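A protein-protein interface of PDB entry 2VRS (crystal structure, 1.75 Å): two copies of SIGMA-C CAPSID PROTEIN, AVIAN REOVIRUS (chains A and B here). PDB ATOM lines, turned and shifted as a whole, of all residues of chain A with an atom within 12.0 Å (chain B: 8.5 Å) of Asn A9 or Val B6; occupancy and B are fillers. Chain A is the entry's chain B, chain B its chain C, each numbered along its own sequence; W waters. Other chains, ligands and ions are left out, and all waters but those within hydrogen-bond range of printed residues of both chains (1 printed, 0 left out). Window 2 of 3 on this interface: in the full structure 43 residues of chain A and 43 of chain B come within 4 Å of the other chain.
Among the printed residues, merely in contact across the chains: Asn A9 with Ser B10 (3.6 Å), Asn A9 with Asn B9 (3.7 Å), Leu A16 with Ile B13 (3.8 Å), Asn A9 with Ile B13 (3.8 Å), Ile A13 with Ile B13 (3.9 Å) and Ala A12 with Ile B13 (3.9 Å).
Asn A9 touches its own counterpart, Asn B9. Asn A9 touches Ser B10, but with the chains exchanged Ser A10 does not touch Asn B9 (8.0 Å). Asn A9 touches Ile B13, but with the chains exchanged Ile A13 does not touch Asn B9 (6.4 Å). Ala A12 touches Ile B13, but with the chains exchanged Ile A13 does not touch Ala B12 (8.0 Å). Of the 7 pairs that touch across the chains among the printed residues, 2 have their exchanged pair printed and touching as well.
ND2 of Asn A9 lies within hydrogen-bond range of O of Val B6 (2.9 Å).
The side-chain hydroxyl of Ser B14 is in hydrogen-bond range of the backbone carbonyl oxygen of Ser B10, 3.0 Å away.
Water W1 lies within hydrogen-bond range of the side-chain amide oxygen of Asn A9 (2.7 Å) and the side-chain hydroxyl of Ser B10 (3.4 Å).
Of chain B, only Val B6, Asn B9, Ser B10 and Ile B13 come within 4 Å of Asn A9. Val B6 touches just one residue of chain A: Asn A9. Gly A8 touches none of the printed residues of chain B. No residue of chain B comes within 4 Å of Ser A10. No residue of chain A comes within 4 Å of Leu B2. Thr B5 touches none of the printed residues of chain A. No residue of chain A comes within 4 Å of Asp B7. Asn B9 touches one residue of chain A. Of chain A, only Asn A9 comes within 4 Å of Ser B10. Of the printed residues of chain B, Ile A13 touches Ile B13. Of the printed residues of chain B, Ala A12 touches Ile B13. Ile A20 touches none of the printed residues of chain B. Ser B14 touches none of the printed residues of chain A. The nearest residue of chain B that does not touch Asn A9 is Thr B5 (5.0 Å). The nearest residue of chain A that does not touch Val B6 is Asp A7 (5.6 Å).
Among the printed residues, no Asp or Glu carboxylate lies within 4 Å of a Lys or Arg side-chain nitrogen of the other chain.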
ATOM      1  N   ASP A   7      -2.546  -3.899 -18.998  1.00  0.00           N
ATOM      2  CA  ASP A   7      -2.554  -2.813 -20.034  1.00  0.00           C
ATOM      3  C   ASP A   7      -1.819  -1.516 -19.621  1.00  0.00           C
ATOM      4  O   ASP A   7      -1.058  -0.963 -20.418  1.00  0.00           O
ATOM      5  CB  ASP A   7      -3.973  -2.502 -20.491  1.00  0.00           C
ATOM      6  CG  ASP A   7      -4.028  -1.324 -21.446  1.00  0.00           C
ATOM      7  OD1 ASP A   7      -4.298  -0.183 -21.008  1.00  0.00           O
ATOM      8  OD2 ASP A   7      -3.780  -1.533 -22.646  1.00  0.00           O
ATOM      9  N   GLY A   8      -2.048  -1.027 -18.398  1.00  0.00           N
ATOM     10  CA  GLY A   8      -1.186   0.031 -17.835  1.00  0.00           C
ATOM     11  C   GLY A   8       0.247  -0.479 -17.891  1.00  0.00           C
ATOM     12  O   GLY A   8       1.183   0.260 -18.234  1.00  0.00           O
ATOM     13  N   ASN A   9       0.404  -1.766 -17.590  1.00  0.00           N
ATOM     14  CA  ASN A   9       1.713  -2.426 -17.676  1.00  0.00           C
ATOM     15  C   ASN A   9       2.309  -2.342 -19.086  1.00  0.00           C
ATOM     16  O   ASN A   9       3.523  -2.148 -19.226  1.00  0.00           O
ATOM     17  CB  ASN A   9       1.643  -3.879 -17.190  1.00  0.00           C
ATOM     18  CG  ASN A   9       1.572  -3.996 -15.669  1.00  0.00           C
ATOM     19  OD1 ASN A   9       1.895  -3.049 -14.930  1.00  0.00           O
ATOM     20  ND2 ASN A   9       1.190  -5.173 -15.193  1.00  0.00           N
ATOM     21  N   SER A  10       1.465  -2.437 -20.122  1.00  0.00           N
ATOM     22  CA  SER A  10       1.961  -2.400 -21.508  1.00  0.00           C
ATOM     23  C   SER A  10       2.629  -1.079 -21.844  1.00  0.00           C
ATOM     24  O   SER A  10       3.656  -1.072 -22.529  1.00  0.00           O
ATOM     25  CB  SER A  10       0.886  -2.760 -22.561  1.00  0.00           C
ATOM     26  OG  SER A  10      -0.129  -1.760 -22.694  1.00  0.00           O
ATOM     27  N   THR A  11       2.057   0.019 -21.342  1.00  0.00           N
ATOM     28  CA  THR A  11       2.627   1.349 -21.524  1.00  0.00           C
ATOM     29  C   THR A  11       4.004   1.439 -20.859  1.00  0.00           C
ATOM     30  O   THR A  11       4.942   1.994 -21.442  1.00  0.00           O
ATOM     31  CB  THR A  11       1.693   2.452 -20.948  1.00  0.00           C
ATOM     32  OG1 THR A  11       0.409   2.361 -21.589  1.00  0.00           O
ATOM     33  CG2 THR A  11       2.277   3.854 -21.185  1.00  0.00           C
ATOM     34  N   ALA A  12       4.097   0.908 -19.638  1.00  0.00           N
ATOM     35  CA  ALA A  12       5.323   0.894 -18.855  1.00  0.00           C
ATOM     36  C   ALA A  12       6.393   0.068 -19.575  1.00  0.00           C
ATOM     37  O   ALA A  12       7.555   0.461 -19.623  1.00  0.00           O
ATOM     38  CB  ALA A  12       5.057   0.356 -17.463  1.00  0.00           C
ATOM     39  N   ILE A  13       5.987  -1.060 -20.160  1.00  0.00           N
ATOM     40  CA  ILE A  13       6.897  -1.894 -20.973  1.00  0.00           C
ATOM     41  C   ILE A  13       7.419  -1.137 -22.195  1.00  0.00           C
ATOM     42  O   ILE A  13       8.615  -1.183 -22.506  1.00  0.00           O
ATOM     43  CB  ILE A  13       6.222  -3.251 -21.370  1.00  0.00           C
ATOM     44  CG1 ILE A  13       6.253  -4.193 -20.156  1.00  0.00           C
ATOM     45  CG2 ILE A  13       6.920  -3.904 -22.590  1.00  0.00           C
ATOM     46  CD1 ILE A  13       5.142  -5.223 -20.118  1.00  0.00           C
ATOM     47  N   SER A  14       6.517  -0.437 -22.878  1.00  0.00           N
ATOM     48  CA  SER A  14       6.862   0.362 -24.036  1.00  0.00           C
ATOM     49  C   SER A  14       7.850   1.486 -23.659  1.00  0.00           C
ATOM     50  O   SER A  14       8.746   1.831 -24.437  1.00  0.00           O
ATOM     51  CB  SER A  14       5.588   0.941 -24.650  1.00  0.00           C
ATOM     52  OG  SER A  14       5.906   1.982 -25.552  1.00  0.00           O
ATOM     53  N   ASN A  15       7.693   2.040 -22.462  1.00  0.00           N
ATOM     54  CA  ASN A  15       8.582   3.104 -21.995  1.00  0.00           C
ATOM     55  C   ASN A  15       9.963   2.543 -21.672  1.00  0.00           C
ATOM     56  O   ASN A  15      10.979   3.161 -21.982  1.00  0.00           O
ATOM     57  CB  ASN A  15       8.001   3.790 -20.758  1.00  0.00           C
ATOM     58  CG  ASN A  15       6.812   4.713 -21.088  1.00  0.00           C
ATOM     59  OD1 ASN A  15       6.654   5.159 -22.222  1.00  0.00           O
ATOM     60  ND2 ASN A  15       5.978   4.994 -20.083  1.00  0.00           N
ATOM     61  N   LEU A  16       9.984   1.375 -21.036  1.00  0.00           N
ATOM     62  CA  LEU A  16      11.235   0.686 -20.673  1.00  0.00           C
ATOM     63  C   LEU A  16      12.031   0.343 -21.910  1.00  0.00           C
ATOM     64  O   LEU A  16      13.243   0.560 -21.941  1.00  0.00           O
ATOM     65  CB  LEU A  16      10.958  -0.572 -19.824  1.00  0.00           C
ATOM     66  CG  LEU A  16      11.046  -0.378 -18.305  1.00  0.00           C
ATOM     67  CD1 LEU A  16      10.061   0.664 -17.784  1.00  0.00           C
ATOM     68  CD2 LEU A  16      10.909  -1.694 -17.560  1.00  0.00           C
ATOM     69  N   LYS A  17      11.343  -0.147 -22.942  1.00  0.00           N
ATOM     70  CA  LYS A  17      11.971  -0.500 -24.209  1.00  0.00           C
ATOM     71  C   LYS A  17      12.756   0.676 -24.774  1.00  0.00           C
ATOM     72  O   LYS A  17      13.869   0.510 -25.291  1.00  0.00           O
ATOM     73  CB  LYS A  17      10.929  -0.926 -25.237  1.00  0.00           C
ATOM     74  CG  LYS A  17      10.534  -2.377 -25.201  1.00  0.00           C
ATOM     75  CD  LYS A  17       9.630  -2.700 -26.397  1.00  0.00           C
ATOM     76  CE  LYS A  17       8.970  -4.059 -26.249  1.00  0.00           C
ATOM     77  NZ  LYS A  17       7.845  -4.258 -27.209  1.00  0.00           N
ATOM     78  N   SER A  18      12.166   1.864 -24.680  1.00  0.00           N
ATOM     79  CA  SER A  18      12.763   3.047 -25.267  1.00  0.00           C
ATOM     80  C   SER A  18      14.064   3.422 -24.533  1.00  0.00           C
ATOM     81  O   SER A  18      15.089   3.754 -25.167  1.00  0.00           O
ATOM     82  CB  SER A  18      11.755   4.197 -25.243  1.00  0.00           C
ATOM     83  OG  SER A  18      12.184   5.217 -26.114  1.00  0.00           O
ATOM     84  N   ILE A  20      15.954   1.271 -22.687  1.00  0.00           N
ATOM     85  CA  ILE A  20      16.920   0.191 -23.002  1.00  0.00           C
ATOM     86  C   ILE A  20      17.590   0.463 -24.332  1.00  0.00           C
ATOM     87  O   ILE A  20      18.816   0.284 -24.487  1.00  0.00           O
ATOM     88  CB  ILE A  20      16.218  -1.211 -23.020  1.00  0.00           C
ATOM     89  CG1 ILE A  20      15.796  -1.585 -21.612  1.00  0.00           C
ATOM     90  CG2 ILE A  20      17.116  -2.331 -23.709  1.00  0.00           C
ATOM     91  CD1 ILE A  20      14.640  -2.634 -21.584  1.00  0.00           C
ATOM     92  N   LEU B   2      -5.890 -13.240 -12.207  1.00  0.00           N
ATOM     93  CA  LEU B   2      -5.690 -12.074 -13.130  1.00  0.00           C
ATOM     94  C   LEU B   2      -5.215 -10.802 -12.421  1.00  0.00           C
ATOM     95  O   LEU B   2      -4.303 -10.149 -12.921  1.00  0.00           O
ATOM     96  CB  LEU B   2      -6.936 -11.789 -13.985  1.00  0.00           C
ATOM     97  CG  LEU B   2      -6.815 -10.773 -15.137  1.00  0.00           C
ATOM     98  CD1 LEU B   2      -6.005 -11.327 -16.317  1.00  0.00           C
ATOM     99  CD2 LEU B   2      -8.190 -10.302 -15.614  1.00  0.00           C
ATOM    100  N   GLN B   3      -5.823 -10.442 -11.280  1.00  0.00           N
ATOM    101  CA  GLN B   3      -5.308  -9.313 -10.456  1.00  0.00           C
ATOM    102  C   GLN B   3      -3.845  -9.543 -10.059  1.00  0.00           C
ATOM    103  O   GLN B   3      -3.018  -8.625 -10.112  1.00  0.00           O
ATOM    104  CB  GLN B   3      -6.174  -9.069  -9.199  1.00  0.00           C
ATOM    105  CG  GLN B   3      -7.652  -8.706  -9.495  1.00  0.00           C
ATOM    106  CD  GLN B   3      -7.786  -7.473 -10.393  1.00  0.00           C
ATOM    107  OE1 GLN B   3      -7.855  -7.582 -11.615  1.00  0.00           O
ATOM    108  NE2 GLN B   3      -7.794  -6.302  -9.787  1.00  0.00           N
ATOM    109  N   THR B   4      -3.521 -10.786  -9.694  1.00  0.00           N
ATOM    110  CA  THR B   4      -2.164 -11.149  -9.253  1.00  0.00           C
ATOM    111  C   THR B   4      -1.153 -11.087 -10.386  1.00  0.00           C
ATOM    112  O   THR B   4       0.010 -10.734 -10.169  1.00  0.00           O
ATOM    113  CB  THR B   4      -2.154 -12.585  -8.725  1.00  0.00           C
ATOM    114  OG1 THR B   4      -2.943 -13.404  -9.622  1.00  0.00           O
ATOM    115  CG2 THR B   4      -2.738 -12.614  -7.306  1.00  0.00           C
ATOM    116  N   THR B   5      -1.602 -11.464 -11.581  1.00  0.00           N
ATOM    117  CA  THR B   5      -0.784 -11.374 -12.805  1.00  0.00           C
ATOM    118  C   THR B   5      -0.306  -9.934 -13.002  1.00  0.00           C
ATOM    119  O   THR B   5       0.892  -9.659 -13.033  1.00  0.00           O
ATOM    120  CB  THR B   5      -1.586 -11.837 -14.047  1.00  0.00           C
ATOM    121  OG1 THR B   5      -2.085 -13.165 -13.815  1.00  0.00           O
ATOM    122  CG2 THR B   5      -0.709 -11.803 -15.329  1.00  0.00           C
ATOM    123  N   VAL B   6      -1.274  -9.029 -13.106  1.00  0.00           N
ATOM    124  CA  VAL B   6      -1.039  -7.603 -13.334  1.00  0.00           C
ATOM    125  C   VAL B   6      -0.181  -6.975 -12.215  1.00  0.00           C
ATOM    126  O   VAL B   6       0.735  -6.158 -12.465  1.00  0.00           O
ATOM    127  CB  VAL B   6      -2.395  -6.882 -13.435  1.00  0.00           C
ATOM    128  CG1 VAL B   6      -2.219  -5.362 -13.584  1.00  0.00           C
ATOM    129  CG2 VAL B   6      -3.248  -7.475 -14.583  1.00  0.00           C
ATOM    130  N   ASP B   7      -0.461  -7.361 -10.971  1.00  0.00           N
ATOM    131  CA  ASP B   7       0.263  -6.768  -9.857  1.00  0.00           C
ATOM    132  C   ASP B   7       1.695  -7.308  -9.795  1.00  0.00           C
ATOM    133  O   ASP B   7       2.638  -6.552  -9.541  1.00  0.00           O
ATOM    134  CB  ASP B   7      -0.462  -7.011  -8.537  1.00  0.00           C
ATOM    135  CG  ASP B   7       0.139  -6.220  -7.399  1.00  0.00           C
ATOM    136  OD1 ASP B   7      -0.203  -5.026  -7.263  1.00  0.00           O
ATOM    137  OD2 ASP B   7       0.942  -6.786  -6.627  1.00  0.00           O
ATOM    138  N   GLY B   8       1.853  -8.604 -10.061  1.00  0.00           N
ATOM    139  CA  GLY B   8       3.183  -9.231 -10.070  1.00  0.00           C
ATOM    140  C   GLY B   8       4.068  -8.706 -11.190  1.00  0.00           C
ATOM    141  O   GLY B   8       5.271  -8.451 -10.992  1.00  0.00           O
ATOM    142  N   ASN B   9       3.473  -8.569 -12.369  1.00  0.00           N
ATOM    143  CA  ASN B   9       4.171  -8.007 -13.514  1.00  0.00           C
ATOM    144  C   ASN B   9       4.618  -6.584 -13.256  1.00  0.00           C
ATOM    145  O   ASN B   9       5.732  -6.215 -13.617  1.00  0.00           O
ATOM    146  CB  ASN B   9       3.316  -8.108 -14.749  1.00  0.00           C
ATOM    147  CG  ASN B   9       3.309  -9.519 -15.323  1.00  0.00           C
ATOM    148  OD1 ASN B   9       4.163 -10.340 -14.970  1.00  0.00           O
ATOM    149  ND2 ASN B   9       2.372  -9.798 -16.223  1.00  0.00           N
ATOM    150  N   SER B  10       3.772  -5.799 -12.581  1.00  0.00           N
ATOM    151  CA  SER B  10       4.139  -4.435 -12.180  1.00  0.00           C
ATOM    152  C   SER B  10       5.377  -4.370 -11.270  1.00  0.00           C
ATOM    153  O   SER B  10       6.256  -3.519 -11.483  1.00  0.00           O
ATOM    154  CB  SER B  10       2.949  -3.735 -11.512  1.00  0.00           C
ATOM    155  OG  SER B  10       3.312  -2.414 -11.143  1.00  0.00           O
ATOM    156  N   THR B  11       5.451  -5.246 -10.268  1.00  0.00           N
ATOM    157  CA  THR B  11       6.641  -5.343  -9.411  1.00  0.00           C
ATOM    158  C   THR B  11       7.914  -5.687 -10.222  1.00  0.00           C
ATOM    159  O   THR B  11       8.972  -5.085 -10.009  1.00  0.00           O
ATOM    160  CB  THR B  11       6.468  -6.384  -8.319  1.00  0.00           C
ATOM    161  OG1 THR B  11       5.275  -6.102  -7.585  1.00  0.00           O
ATOM    162  CG2 THR B  11       7.654  -6.356  -7.359  1.00  0.00           C
ATOM    163  N   ALA B  12       7.795  -6.662 -11.118  1.00  0.00           N
ATOM    164  CA  ALA B  12       8.888  -7.022 -12.043  1.00  0.00           C
ATOM    165  C   ALA B  12       9.325  -5.832 -12.898  1.00  0.00           C
ATOM    166  O   ALA B  12      10.525  -5.550 -13.035  1.00  0.00           O
ATOM    167  CB  ALA B  12       8.466  -8.220 -12.918  1.00  0.00           C
ATOM    168  N   ILE B  13       8.362  -5.121 -13.474  1.00  0.00           N
ATOM    169  CA  ILE B  13       8.649  -3.895 -14.231  1.00  0.00           C
ATOM    170  C   ILE B  13       9.427  -2.854 -13.384  1.00  0.00           C
ATOM    171  O   ILE B  13      10.402  -2.259 -13.870  1.00  0.00           O
ATOM    172  CB  ILE B  13       7.358  -3.320 -14.883  1.00  0.00           C
ATOM    173  CG1 ILE B  13       6.899  -4.224 -16.031  1.00  0.00           C
ATOM    174  CG2 ILE B  13       7.530  -1.859 -15.365  1.00  0.00           C
ATOM    175  CD1 ILE B  13       5.379  -4.082 -16.375  1.00  0.00           C
ATOM    176  N   SER B  14       9.029  -2.653 -12.128  1.00  0.00           N
ATOM    177  CA  SER B  14       9.718  -1.710 -11.228  1.00  0.00           C
ATOM    178  C   SER B  14      11.173  -2.126 -10.979  1.00  0.00           C
ATOM    179  O   SER B  14      12.076  -1.288 -10.919  1.00  0.00           O
ATOM    180  CB  SER B  14       8.967  -1.566  -9.902  1.00  0.00           C
ATOM    181  OG  SER B  14       7.621  -1.184 -10.172  1.00  0.00           O
HETATM  182  O   HOH W   1       3.184  -0.766 -14.156  1.00  0.00           O
